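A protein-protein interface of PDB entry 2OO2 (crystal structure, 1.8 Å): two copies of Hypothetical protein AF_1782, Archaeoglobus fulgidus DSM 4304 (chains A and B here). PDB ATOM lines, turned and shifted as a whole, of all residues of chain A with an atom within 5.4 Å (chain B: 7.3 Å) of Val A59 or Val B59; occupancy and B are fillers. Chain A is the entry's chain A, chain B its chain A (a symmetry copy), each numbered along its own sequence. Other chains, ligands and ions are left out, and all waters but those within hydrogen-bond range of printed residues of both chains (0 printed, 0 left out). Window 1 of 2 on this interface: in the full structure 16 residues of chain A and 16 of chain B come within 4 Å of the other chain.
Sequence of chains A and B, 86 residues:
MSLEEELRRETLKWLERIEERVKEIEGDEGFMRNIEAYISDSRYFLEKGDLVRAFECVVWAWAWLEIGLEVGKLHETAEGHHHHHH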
ATOM      1  N   PHE A  55      26.466 -23.612 -16.437  1.00  0.00           N
ATOM      2  CA  PHE A  55      25.780 -23.869 -17.691  1.00  0.00           C
ATOM      3  C   PHE A  55      26.767 -24.100 -18.840  1.00  0.00           C
ATOM      4  O   PHE A  55      26.614 -25.084 -19.668  1.00  0.00           O
ATOM      5  CB  PHE A  55      24.855 -22.747 -18.044  1.00  0.00           C
ATOM      6  CG  PHE A  55      24.026 -22.953 -19.277  1.00  0.00           C
ATOM      7  CD1 PHE A  55      23.037 -23.926 -19.363  1.00  0.00           C
ATOM      8  CD2 PHE A  55      24.240 -22.056 -20.364  1.00  0.00           C
ATOM      9  CE1 PHE A  55      22.241 -24.015 -20.507  1.00  0.00           C
ATOM     10  CE2 PHE A  55      23.355 -22.102 -21.515  1.00  0.00           C
ATOM     11  CZ  PHE A  55      22.389 -23.119 -21.558  1.00  0.00           C
ATOM     12  N   GLU A  56      27.802 -23.266 -18.907  1.00  0.00           N
ATOM     13  CA  GLU A  56      28.819 -23.355 -19.938  1.00  0.00           C
ATOM     14  C   GLU A  56      29.375 -24.790 -19.925  1.00  0.00           C
ATOM     15  O   GLU A  56      29.559 -25.437 -21.038  1.00  0.00           O
ATOM     16  CB  GLU A  56      29.916 -22.375 -19.595  1.00  0.00           C
ATOM     17  CG  GLU A  56      30.948 -22.187 -20.730  1.00  0.00           C
ATOM     18  CD  GLU A  56      32.137 -21.315 -20.359  1.00  0.00           C
ATOM     19  OE1 GLU A  56      32.593 -21.262 -19.215  1.00  0.00           O
ATOM     20  OE2 GLU A  56      32.640 -20.669 -21.250  1.00  0.00           O
ATOM     21  N   CYS A  57      29.687 -25.331 -18.749  1.00  0.00           N
ATOM     22  CA  CYS A  57      30.306 -26.760 -18.717  1.00  0.00           C
ATOM     23  C   CYS A  57      29.309 -27.827 -19.145  1.00  0.00           C
ATOM     24  O   CYS A  57      29.746 -28.835 -19.940  1.00  0.00           O
ATOM     25  CB  CYS A  57      30.997 -27.072 -17.351  1.00  0.00           C
ATOM     26  SG  CYS A  57      32.359 -26.057 -16.966  1.00  0.00           S
ATOM     27  N   VAL A  58      28.009 -27.751 -18.805  1.00  0.00           N
ATOM     28  CA  VAL A  58      26.984 -28.724 -19.222  1.00  0.00           C
ATOM     29  C   VAL A  58      26.832 -28.775 -20.785  1.00  0.00           C
ATOM     30  O   VAL A  58      26.811 -29.913 -21.410  1.00  0.00           O
ATOM     31  CB  VAL A  58      25.637 -28.658 -18.436  1.00  0.00           C
ATOM     32  CG1 VAL A  58      24.685 -27.659 -19.044  1.00  0.00           C
ATOM     33  CG2 VAL A  58      24.987 -30.099 -18.452  1.00  0.00           C
ATOM     34  N   VAL A  59      26.945 -27.599 -21.425  1.00  0.00           N
ATOM     35  CA  VAL A  59      26.783 -27.483 -22.883  1.00  0.00           C
ATOM     36  C   VAL A  59      28.038 -28.135 -23.448  1.00  0.00           C
ATOM     37  O   VAL A  59      27.872 -28.957 -24.390  1.00  0.00           O
ATOM     38  CB  VAL A  59      26.765 -26.102 -23.347  1.00  0.00           C
ATOM     39  CG1 VAL A  59      26.589 -26.011 -24.787  1.00  0.00           C
ATOM     40  CG2 VAL A  59      25.429 -25.425 -22.751  1.00  0.00           C
ATOM     41  N   TRP A  60      29.228 -27.762 -22.953  1.00  0.00           N
ATOM     42  CA  TRP A  60      30.477 -28.477 -23.482  1.00  0.00           C
ATOM     43  C   TRP A  60      30.331 -29.962 -23.285  1.00  0.00           C
ATOM     44  O   TRP A  60      30.765 -30.756 -24.230  1.00  0.00           O
ATOM     45  CB  TRP A  60      31.776 -27.977 -22.806  1.00  0.00           C
ATOM     46  CG  TRP A  60      32.330 -26.737 -23.492  1.00  0.00           C
ATOM     47  CD1 TRP A  60      32.134 -25.411 -23.109  1.00  0.00           C
ATOM     48  CD2 TRP A  60      33.070 -26.683 -24.700  1.00  0.00           C
ATOM     49  NE1 TRP A  60      32.793 -24.555 -23.905  1.00  0.00           N
ATOM     50  CE2 TRP A  60      33.365 -25.311 -24.948  1.00  0.00           C
ATOM     51  CE3 TRP A  60      33.523 -27.675 -25.615  1.00  0.00           C
ATOM     52  CZ2 TRP A  60      34.031 -24.875 -26.064  1.00  0.00           C
ATOM     53  CZ3 TRP A  60      34.255 -27.243 -26.702  1.00  0.00           C
ATOM     54  CH2 TRP A  60      34.513 -25.869 -26.945  1.00  0.00           C
ATOM     55  N   ALA A  61      29.897 -30.408 -22.092  1.00  0.00           N
ATOM     56  CA  ALA A  61      29.725 -31.899 -21.899  1.00  0.00           C
ATOM     57  C   ALA A  61      28.814 -32.537 -22.980  1.00  0.00           C
ATOM     58  O   ALA A  61      29.215 -33.567 -23.670  1.00  0.00           O
ATOM     59  CB  ALA A  61      29.255 -32.254 -20.474  1.00  0.00           C
ATOM     60  N   TRP A  62      27.663 -31.905 -23.219  1.00  0.00           N
ATOM     61  CA  TRP A  62      26.765 -32.363 -24.274  1.00  0.00           C
ATOM     62  C   TRP A  62      27.344 -32.323 -25.705  1.00  0.00           C
ATOM     63  O   TRP A  62      27.069 -33.252 -26.514  1.00  0.00           O
ATOM     64  CB  TRP A  62      25.444 -31.598 -24.187  1.00  0.00           C
ATOM     65  CG  TRP A  62      24.510 -32.254 -23.241  1.00  0.00           C
ATOM     66  CD1 TRP A  62      24.100 -31.770 -21.976  1.00  0.00           C
ATOM     67  CD2 TRP A  62      23.794 -33.485 -23.437  1.00  0.00           C
ATOM     68  NE1 TRP A  62      23.231 -32.647 -21.430  1.00  0.00           N
ATOM     69  CE2 TRP A  62      22.988 -33.691 -22.294  1.00  0.00           C
ATOM     70  CE3 TRP A  62      23.751 -34.444 -24.487  1.00  0.00           C
ATOM     71  CZ2 TRP A  62      22.170 -34.823 -22.142  1.00  0.00           C
ATOM     72  CZ3 TRP A  62      22.934 -35.535 -24.337  1.00  0.00           C
ATOM     73  CH2 TRP A  62      22.173 -35.738 -23.174  1.00  0.00           C
ATOM     74  N   ALA A  63      28.160 -31.298 -26.018  1.00  0.00           N
ATOM     75  CA  ALA A  63      28.707 -31.166 -27.360  1.00  0.00           C
ATOM     76  C   ALA A  63      29.711 -32.309 -27.594  1.00  0.00           C
ATOM     77  O   ALA A  63      29.720 -32.854 -28.688  1.00  0.00           O
ATOM     78  CB  ALA A  63      29.408 -29.836 -27.600  1.00  0.00           C
ATOM     79  N   TRP A  64      30.563 -32.624 -26.624  1.00  0.00           N
ATOM     80  CA  TRP A  64      31.583 -33.728 -26.786  1.00  0.00           C
ATOM     81  C   TRP A  64      30.826 -35.031 -26.998  1.00  0.00           C
ATOM     82  O   TRP A  64      31.263 -35.898 -27.832  1.00  0.00           O
ATOM     83  CB  TRP A  64      32.512 -33.873 -25.574  1.00  0.00           C
ATOM     84  CG  TRP A  64      33.662 -32.876 -25.623  1.00  0.00           C
ATOM     85  CD1 TRP A  64      33.701 -31.650 -25.012  1.00  0.00           C
ATOM     86  CD2 TRP A  64      34.856 -32.994 -26.389  1.00  0.00           C
ATOM     87  NE1 TRP A  64      34.886 -30.998 -25.341  1.00  0.00           N
ATOM     88  CE2 TRP A  64      35.607 -31.809 -26.191  1.00  0.00           C
ATOM     89  CE3 TRP A  64      35.378 -34.004 -27.229  1.00  0.00           C
ATOM     90  CZ2 TRP A  64      36.855 -31.599 -26.807  1.00  0.00           C
ATOM     91  CZ3 TRP A  64      36.640 -33.799 -27.817  1.00  0.00           C
ATOM     92  CH2 TRP A  64      37.347 -32.617 -27.618  1.00  0.00           C
ATOM     93  N   TRP B  14      32.839 -13.924 -26.872  1.00  0.00           N
ATOM     94  CA  TRP B  14      33.088 -15.222 -27.581  1.00  0.00           C
ATOM     95  C   TRP B  14      32.522 -15.189 -28.984  1.00  0.00           C
ATOM     96  O   TRP B  14      32.974 -15.944 -29.948  1.00  0.00           O
ATOM     97  CB  TRP B  14      32.485 -16.269 -26.707  1.00  0.00           C
ATOM     98  CG  TRP B  14      33.382 -16.615 -25.572  1.00  0.00           C
ATOM     99  CD1 TRP B  14      33.111 -16.509 -24.241  1.00  0.00           C
ATOM    100  CD2 TRP B  14      34.701 -17.150 -25.670  1.00  0.00           C
ATOM    101  NE1 TRP B  14      34.183 -16.915 -23.495  1.00  0.00           N
ATOM    102  CE2 TRP B  14      35.166 -17.354 -24.368  1.00  0.00           C
ATOM    103  CE3 TRP B  14      35.543 -17.493 -26.772  1.00  0.00           C
ATOM    104  CZ2 TRP B  14      36.446 -17.838 -24.105  1.00  0.00           C
ATOM    105  CZ3 TRP B  14      36.807 -17.982 -26.511  1.00  0.00           C
ATOM    106  CH2 TRP B  14      37.255 -18.168 -25.204  1.00  0.00           C
ATOM    107  N   ILE B  18      34.657 -15.602 -32.416  1.00  0.00           N
ATOM    108  CA  ILE B  18      34.387 -16.713 -33.383  1.00  0.00           C
ATOM    109  C   ILE B  18      34.081 -16.189 -34.795  1.00  0.00           C
ATOM    110  O   ILE B  18      34.395 -16.824 -35.835  1.00  0.00           O
ATOM    111  CB  ILE B  18      33.289 -17.659 -32.828  1.00  0.00           C
ATOM    112  CG1 ILE B  18      33.395 -19.018 -33.515  1.00  0.00           C
ATOM    113  CG2 ILE B  18      31.834 -17.049 -32.888  1.00  0.00           C
ATOM    114  CD1 ILE B  18      32.433 -20.106 -32.901  1.00  0.00           C
ATOM    115  N   TYR B  38      24.957 -21.955 -35.734  1.00  0.00           N
ATOM    116  CA  TYR B  38      24.844 -21.433 -34.265  1.00  0.00           C
ATOM    117  C   TYR B  38      25.368 -20.067 -34.121  1.00  0.00           C
ATOM    118  O   TYR B  38      24.771 -19.203 -33.234  1.00  0.00           O
ATOM    119  CB  TYR B  38      25.652 -22.362 -33.336  1.00  0.00           C
ATOM    120  CG  TYR B  38      25.025 -23.697 -33.064  1.00  0.00           C
ATOM    121  CD1 TYR B  38      23.968 -23.832 -32.235  1.00  0.00           C
ATOM    122  CD2 TYR B  38      25.549 -24.899 -33.638  1.00  0.00           C
ATOM    123  CE1 TYR B  38      23.400 -25.005 -31.910  1.00  0.00           C
ATOM    124  CE2 TYR B  38      24.971 -26.158 -33.307  1.00  0.00           C
ATOM    125  CZ  TYR B  38      23.900 -26.219 -32.466  1.00  0.00           C
ATOM    126  OH  TYR B  38      23.240 -27.410 -32.083  1.00  0.00           O
ATOM    127  N   SER B  42      23.153 -17.527 -32.273  1.00  0.00           N
ATOM    128  CA  SER B  42      23.608 -16.671 -31.079  1.00  0.00           C
ATOM    129  C   SER B  42      23.362 -15.176 -31.289  1.00  0.00           C
ATOM    130  O   SER B  42      22.827 -14.428 -30.319  1.00  0.00           O
ATOM    131  CB  SER B  42      25.093 -16.977 -30.859  1.00  0.00           C
ATOM    132  OG  SER B  42      25.706 -16.185 -29.859  1.00  0.00           O
ATOM    133  N   VAL B  52      20.277 -16.516 -22.325  1.00  0.00           N
ATOM    134  CA  VAL B  52      20.641 -17.923 -22.058  1.00  0.00           C
ATOM    135  C   VAL B  52      20.789 -18.623 -23.425  1.00  0.00           C
ATOM    136  O   VAL B  52      21.808 -19.364 -23.663  1.00  0.00           O
ATOM    137  CB  VAL B  52      19.571 -18.678 -21.286  1.00  0.00           C
ATOM    138  CG1 VAL B  52      20.006 -20.030 -20.951  1.00  0.00           C
ATOM    139  CG2 VAL B  52      19.328 -17.983 -19.903  1.00  0.00           C
ATOM    140  N   ARG B  53      19.798 -18.427 -24.309  1.00  0.00           N
ATOM    141  CA  ARG B  53      19.904 -19.147 -25.658  1.00  0.00           C
ATOM    142  C   ARG B  53      21.033 -18.498 -26.429  1.00  0.00           C
ATOM    143  O   ARG B  53      21.803 -19.200 -27.166  1.00  0.00           O
ATOM    144  CB  ARG B  53      18.612 -19.125 -26.468  1.00  0.00           C
ATOM    145  CG  ARG B  53      17.382 -19.767 -25.837  1.00  0.00           C
ATOM    146  CD  ARG B  53      17.406 -21.283 -25.767  1.00  0.00           C
ATOM    147  NE  ARG B  53      17.919 -21.749 -24.462  1.00  0.00           N
ATOM    148  CZ  ARG B  53      17.735 -22.961 -23.946  1.00  0.00           C
ATOM    149  NH1 ARG B  53      18.267 -23.247 -22.767  1.00  0.00           N
ATOM    150  NH2 ARG B  53      17.030 -23.884 -24.604  1.00  0.00           N
ATOM    151  N   ALA B  54      21.235 -17.194 -26.286  1.00  0.00           N
ATOM    152  CA  ALA B  54      22.349 -16.582 -27.001  1.00  0.00           C
ATOM    153  C   ALA B  54      23.672 -17.199 -26.579  1.00  0.00           C
ATOM    154  O   ALA B  54      24.493 -17.490 -27.437  1.00  0.00           O
ATOM    155  CB  ALA B  54      22.439 -15.101 -26.864  1.00  0.00           C
ATOM    156  N   PHE B  55      23.910 -17.310 -25.270  1.00  0.00           N
ATOM    157  CA  PHE B  55      25.139 -17.913 -24.787  1.00  0.00           C
ATOM    158  C   PHE B  55      25.233 -19.394 -25.172  1.00  0.00           C
ATOM    159  O   PHE B  55      26.320 -19.890 -25.670  1.00  0.00           O
ATOM    160  CB  PHE B  55      25.268 -17.773 -23.302  1.00  0.00           C
ATOM    161  CG  PHE B  55      26.548 -18.283 -22.711  1.00  0.00           C
ATOM    162  CD1 PHE B  55      27.781 -17.697 -22.971  1.00  0.00           C
ATOM    163  CD2 PHE B  55      26.456 -19.373 -21.796  1.00  0.00           C
ATOM    164  CE1 PHE B  55      28.928 -18.164 -22.326  1.00  0.00           C
ATOM    165  CE2 PHE B  55      27.638 -19.798 -21.069  1.00  0.00           C
ATOM    166  CZ  PHE B  55      28.860 -19.186 -21.388  1.00  0.00           C
ATOM    167  N   GLU B  56      24.128 -20.118 -25.007  1.00  0.00           N
ATOM    168  CA  GLU B  56      24.061 -21.532 -25.323  1.00  0.00           C
ATOM    169  C   GLU B  56      24.522 -21.710 -26.781  1.00  0.00           C
ATOM    170  O   GLU B  56      25.348 -22.661 -27.100  1.00  0.00           O
ATOM    171  CB  GLU B  56      22.623 -21.972 -25.181  1.00  0.00           C
ATOM    172  CG  GLU B  56      22.440 -23.505 -25.252  1.00  0.00           C
ATOM    173  CD  GLU B  56      20.990 -23.965 -25.253  1.00  0.00           C
ATOM    174  OE1 GLU B  56      20.082 -23.300 -25.754  1.00  0.00           O
ATOM    175  OE2 GLU B  56      20.757 -25.038 -24.745  1.00  0.00           O
ATOM    176  N   CYS B  57      24.029 -20.881 -27.700  1.00  0.00           N
ATOM    177  CA  CYS B  57      24.437 -21.080 -29.189  1.00  0.00           C
ATOM    178  C   CYS B  57      25.904 -20.758 -29.430  1.00  0.00           C
ATOM    179  O   CYS B  57      26.612 -21.564 -30.260  1.00  0.00           O
ATOM    180  CB  CYS B  57      23.473 -20.335 -30.168  1.00  0.00           C
ATOM    181  SG  CYS B  57      21.824 -20.896 -30.145  1.00  0.00           S
ATOM    182  N   VAL B  58      26.516 -19.743 -28.792  1.00  0.00           N
ATOM    183  CA  VAL B  58      27.942 -19.405 -28.944  1.00  0.00           C
ATOM    184  C   VAL B  58      28.872 -20.586 -28.486  1.00  0.00           C
ATOM    185  O   VAL B  58      29.859 -20.979 -29.232  1.00  0.00           O
ATOM    186  CB  VAL B  58      28.360 -17.999 -28.411  1.00  0.00           C
ATOM    187  CG1 VAL B  58      28.707 -18.040 -26.944  1.00  0.00           C
ATOM    188  CG2 VAL B  58      29.609 -17.507 -29.245  1.00  0.00           C
ATOM    189  N   VAL B  59      28.454 -21.280 -27.412  1.00  0.00           N
ATOM    190  CA  VAL B  59      29.241 -22.384 -26.841  1.00  0.00           C
ATOM    191  C   VAL B  59      29.103 -23.504 -27.864  1.00  0.00           C
ATOM    192  O   VAL B  59      30.165 -24.100 -28.193  1.00  0.00           O
ATOM    193  CB  VAL B  59      28.698 -22.879 -25.582  1.00  0.00           C
ATOM    194  CG1 VAL B  59      29.498 -23.958 -25.028  1.00  0.00           C
ATOM    195  CG2 VAL B  59      28.856 -21.689 -24.506  1.00  0.00           C
ATOM    196  N   TRP B  60      27.876 -23.818 -28.305  1.00  0.00           N
ATOM    197  CA  TRP B  60      27.762 -24.899 -29.387  1.00  0.00           C
ATOM    198  C   TRP B  60      28.605 -24.518 -30.574  1.00  0.00           C
ATOM    199  O   TRP B  60      29.269 -25.465 -31.188  1.00  0.00           O
ATOM    200  CB  TRP B  60      26.299 -25.139 -29.829  1.00  0.00           C
ATOM    201  CG  TRP B  60      25.587 -26.129 -28.920  1.00  0.00           C
ATOM    202  CD1 TRP B  60      24.755 -25.827 -27.844  1.00  0.00           C
ATOM    203  CD2 TRP B  60      25.705 -27.542 -28.929  1.00  0.00           C
ATOM    204  NE1 TRP B  60      24.252 -26.931 -27.270  1.00  0.00           N
ATOM    205  CE2 TRP B  60      24.857 -28.039 -27.898  1.00  0.00           C
ATOM    206  CE3 TRP B  60      26.454 -28.456 -29.723  1.00  0.00           C
ATOM    207  CZ2 TRP B  60      24.755 -29.370 -27.582  1.00  0.00           C
ATOM    208  CZ3 TRP B  60      26.298 -29.800 -29.453  1.00  0.00           C
ATOM    209  CH2 TRP B  60      25.470 -30.271 -28.402  1.00  0.00           C
ATOM    210  N   ALA B  61      28.525 -23.258 -31.036  1.00  0.00           N
ATOM    211  CA  ALA B  61      29.390 -22.866 -32.214  1.00  0.00           C
ATOM    212  C   ALA B  61      30.892 -23.164 -31.973  1.00  0.00           C
ATOM    213  O   ALA B  61      31.582 -23.862 -32.832  1.00  0.00           O
ATOM    214  CB  ALA B  61      29.161 -21.404 -32.647  1.00  0.00           C
ATOM    215  N   TRP B  62      31.387 -22.757 -30.802  1.00  0.00           N
ATOM    216  CA  TRP B  62      32.765 -23.060 -30.428  1.00  0.00           C
ATOM    217  C   TRP B  62      33.108 -24.559 -30.306  1.00  0.00           C
ATOM    218  O   TRP B  62      34.232 -24.975 -30.702  1.00  0.00           O
ATOM    219  CB  TRP B  62      33.124 -22.301 -29.150  1.00  0.00           C
ATOM    220  CG  TRP B  62      33.610 -20.935 -29.460  1.00  0.00           C
ATOM    221  CD1 TRP B  62      32.944 -19.714 -29.197  1.00  0.00           C
ATOM    222  CD2 TRP B  62      34.874 -20.571 -30.041  1.00  0.00           C
ATOM    223  NE1 TRP B  62      33.721 -18.691 -29.612  1.00  0.00           N
ATOM    224  CE2 TRP B  62      34.918 -19.159 -30.104  1.00  0.00           C
ATOM    225  CE3 TRP B  62      35.991 -21.314 -30.516  1.00  0.00           C
ATOM    226  CZ2 TRP B  62      36.012 -18.463 -30.646  1.00  0.00           C
ATOM    227  CZ3 TRP B  62      37.060 -20.623 -31.025  1.00  0.00           C
ATOM    228  CH2 TRP B  62      37.064 -19.221 -31.113  1.00  0.00           C
ATOM    229  N   ALA B  63      32.160 -25.376 -29.807  1.00  0.00           N
ATOM    230  CA  ALA B  63      32.426 -26.794 -29.617  1.00  0.00           C
ATOM    231  C   ALA B  63      32.561 -27.456 -31.001  1.00  0.00           C
ATOM    232  O   ALA B  63      33.430 -28.302 -31.154  1.00  0.00           O
ATOM    233  CB  ALA B  63      31.339 -27.515 -28.831  1.00  0.00           C
ATOM    234  N   TRP B  64      31.699 -27.126 -31.958  1.00  0.00           N
ATOM    235  CA  TRP B  64      31.765 -27.742 -33.337  1.00  0.00           C
ATOM    236  C   TRP B  64      33.104 -27.361 -33.951  1.00  0.00           C
ATOM    237  O   TRP B  64      33.751 -28.211 -34.657  1.00  0.00           O
ATOM    238  CB  TRP B  64      30.632 -27.275 -34.260  1.00  0.00           C
ATOM    239  CG  TRP B  64      29.353 -28.065 -34.026  1.00  0.00           C
ATOM    240  CD1 TRP B  64      28.311 -27.703 -33.213  1.00  0.00           C
ATOM    241  CD2 TRP B  64      29.052 -29.363 -34.529  1.00  0.00           C
ATOM    242  NE1 TRP B  64      27.350 -28.710 -33.203  1.00  0.00           N
ATOM    243  CE2 TRP B  64      27.791 -29.740 -34.003  1.00  0.00           C
ATOM    244  CE3 TRP B  64      29.729 -30.254 -35.392  1.00  0.00           C
ATOM    245  CZ2 TRP B  64      27.191 -30.978 -34.307  1.00  0.00           C
ATOM    246  CZ3 TRP B  64      29.109 -31.475 -35.715  1.00  0.00           C
ATOM    247  CH2 TRP B  64      27.878 -31.826 -35.170  1.00  0.00           C
ATOM    248  N   LEU B  65      33.493 -26.097 -33.742  1.00  0.00           N
ATOM    249  CA  LEU B  65      34.781 -25.564 -34.195  1.00  0.00           C
ATOM    250  C   LEU B  65      35.977 -26.242 -33.518  1.00  0.00           C
ATOM    251  O   LEU B  65      36.821 -26.879 -34.243  1.00  0.00           O
ATOM    252  CB  LEU B  65      34.832 -24.018 -34.075  1.00  0.00           C
ATOM    253  CG  LEU B  65      35.979 -23.330 -34.811  1.00  0.00           C
ATOM    254  CD1 LEU B  65      35.664 -21.838 -34.895  1.00  0.00           C
ATOM    255  CD2 LEU B  65      37.317 -23.557 -34.150  1.00  0.00           C
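The indole nitrogen (NE1) of Trp B62 sits at hydrogen-bond distance from the backbone carbonyl oxygen (O) of Trp B14, at 2.9 Å.
The side-chain carboxylate (OE1) of Glu B56 lies within salt-bridge range of the guanidinium group (NE) of Arg B53 (3.0 Å).
O of Val B52 touches CE2 of Phe A55 (3.8 Å).
CG of Glu B56 touches CZ of Phe A55, 3.7 Å away.
Phe B55 touches Glu A56.
Val B59 touches Val A59.
Val A59 touches Trp B60.
Trp A60 touches Val B59.
C of Trp B62 touches CH2 of Trp A60, 3.9 Å away.
CA of Ala B63 touches CZ3 of Trp A60, 3.5 Å away.
C of Trp A62 touches CH2 of Trp B60 (3.9 Å).
Ala A63 touches Trp B60 (CA to CZ3, 3.5 Å).
Val A59 touches just these residues of chain B: Val B59 (3.6 Å) and Trp B60 (3.5 Å).
Of the printed residues of chain B, Trp A62 touches Trp B60 (3.9 Å).
Of the printed residues of chain A, Phe B55 touches Phe A55 and Glu A56.
Printed residues of chain A within 4 Å of Trp B60: Val A59, Trp A62 and Ala A63.
Of the printed residues of chain A, Trp B62 touches Trp A60.
Trp B64 touches none of the printed residues of chain A.
The nearest residue of chain A that does not touch Val B59 is Glu A56 (4.3 Å).
Printed residues of chain A that touch a printed residue of chain B: Phe A55, Glu A56, Val A59, Trp A60, Trp A62 and Ala A63.
Hydrophobic or aromatic side chains of chain A within 4 Å of the printed part of chain B: Phe A55, Val A59, Trp A60 and Ala A63.
Hydrophobic or aromatic side chains of chain B that line the printed part of chain A: Val B52, Phe B55, Val B59, Trp B60 and Ala B63.
Among the printed residues, 12 pairs touch across the chains.
Among the printed residues, no Asp or Glu carboxylate lies within 4 Å of a Lys or Arg side-chain nitrogen of the other chain.
Phe A55 touches Glu B56, and with the chains exchanged Glu A56 touches Phe B55.
Val A59 touches Trp B60, and with the chains exchanged Trp A60 touches Val B59.
Trp A60 touches Trp B62, and with the chains exchanged Trp A62 touches Trp B60.
Trp A60 touches Ala B63, and with the chains exchanged Ala A63 touches Trp B60.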
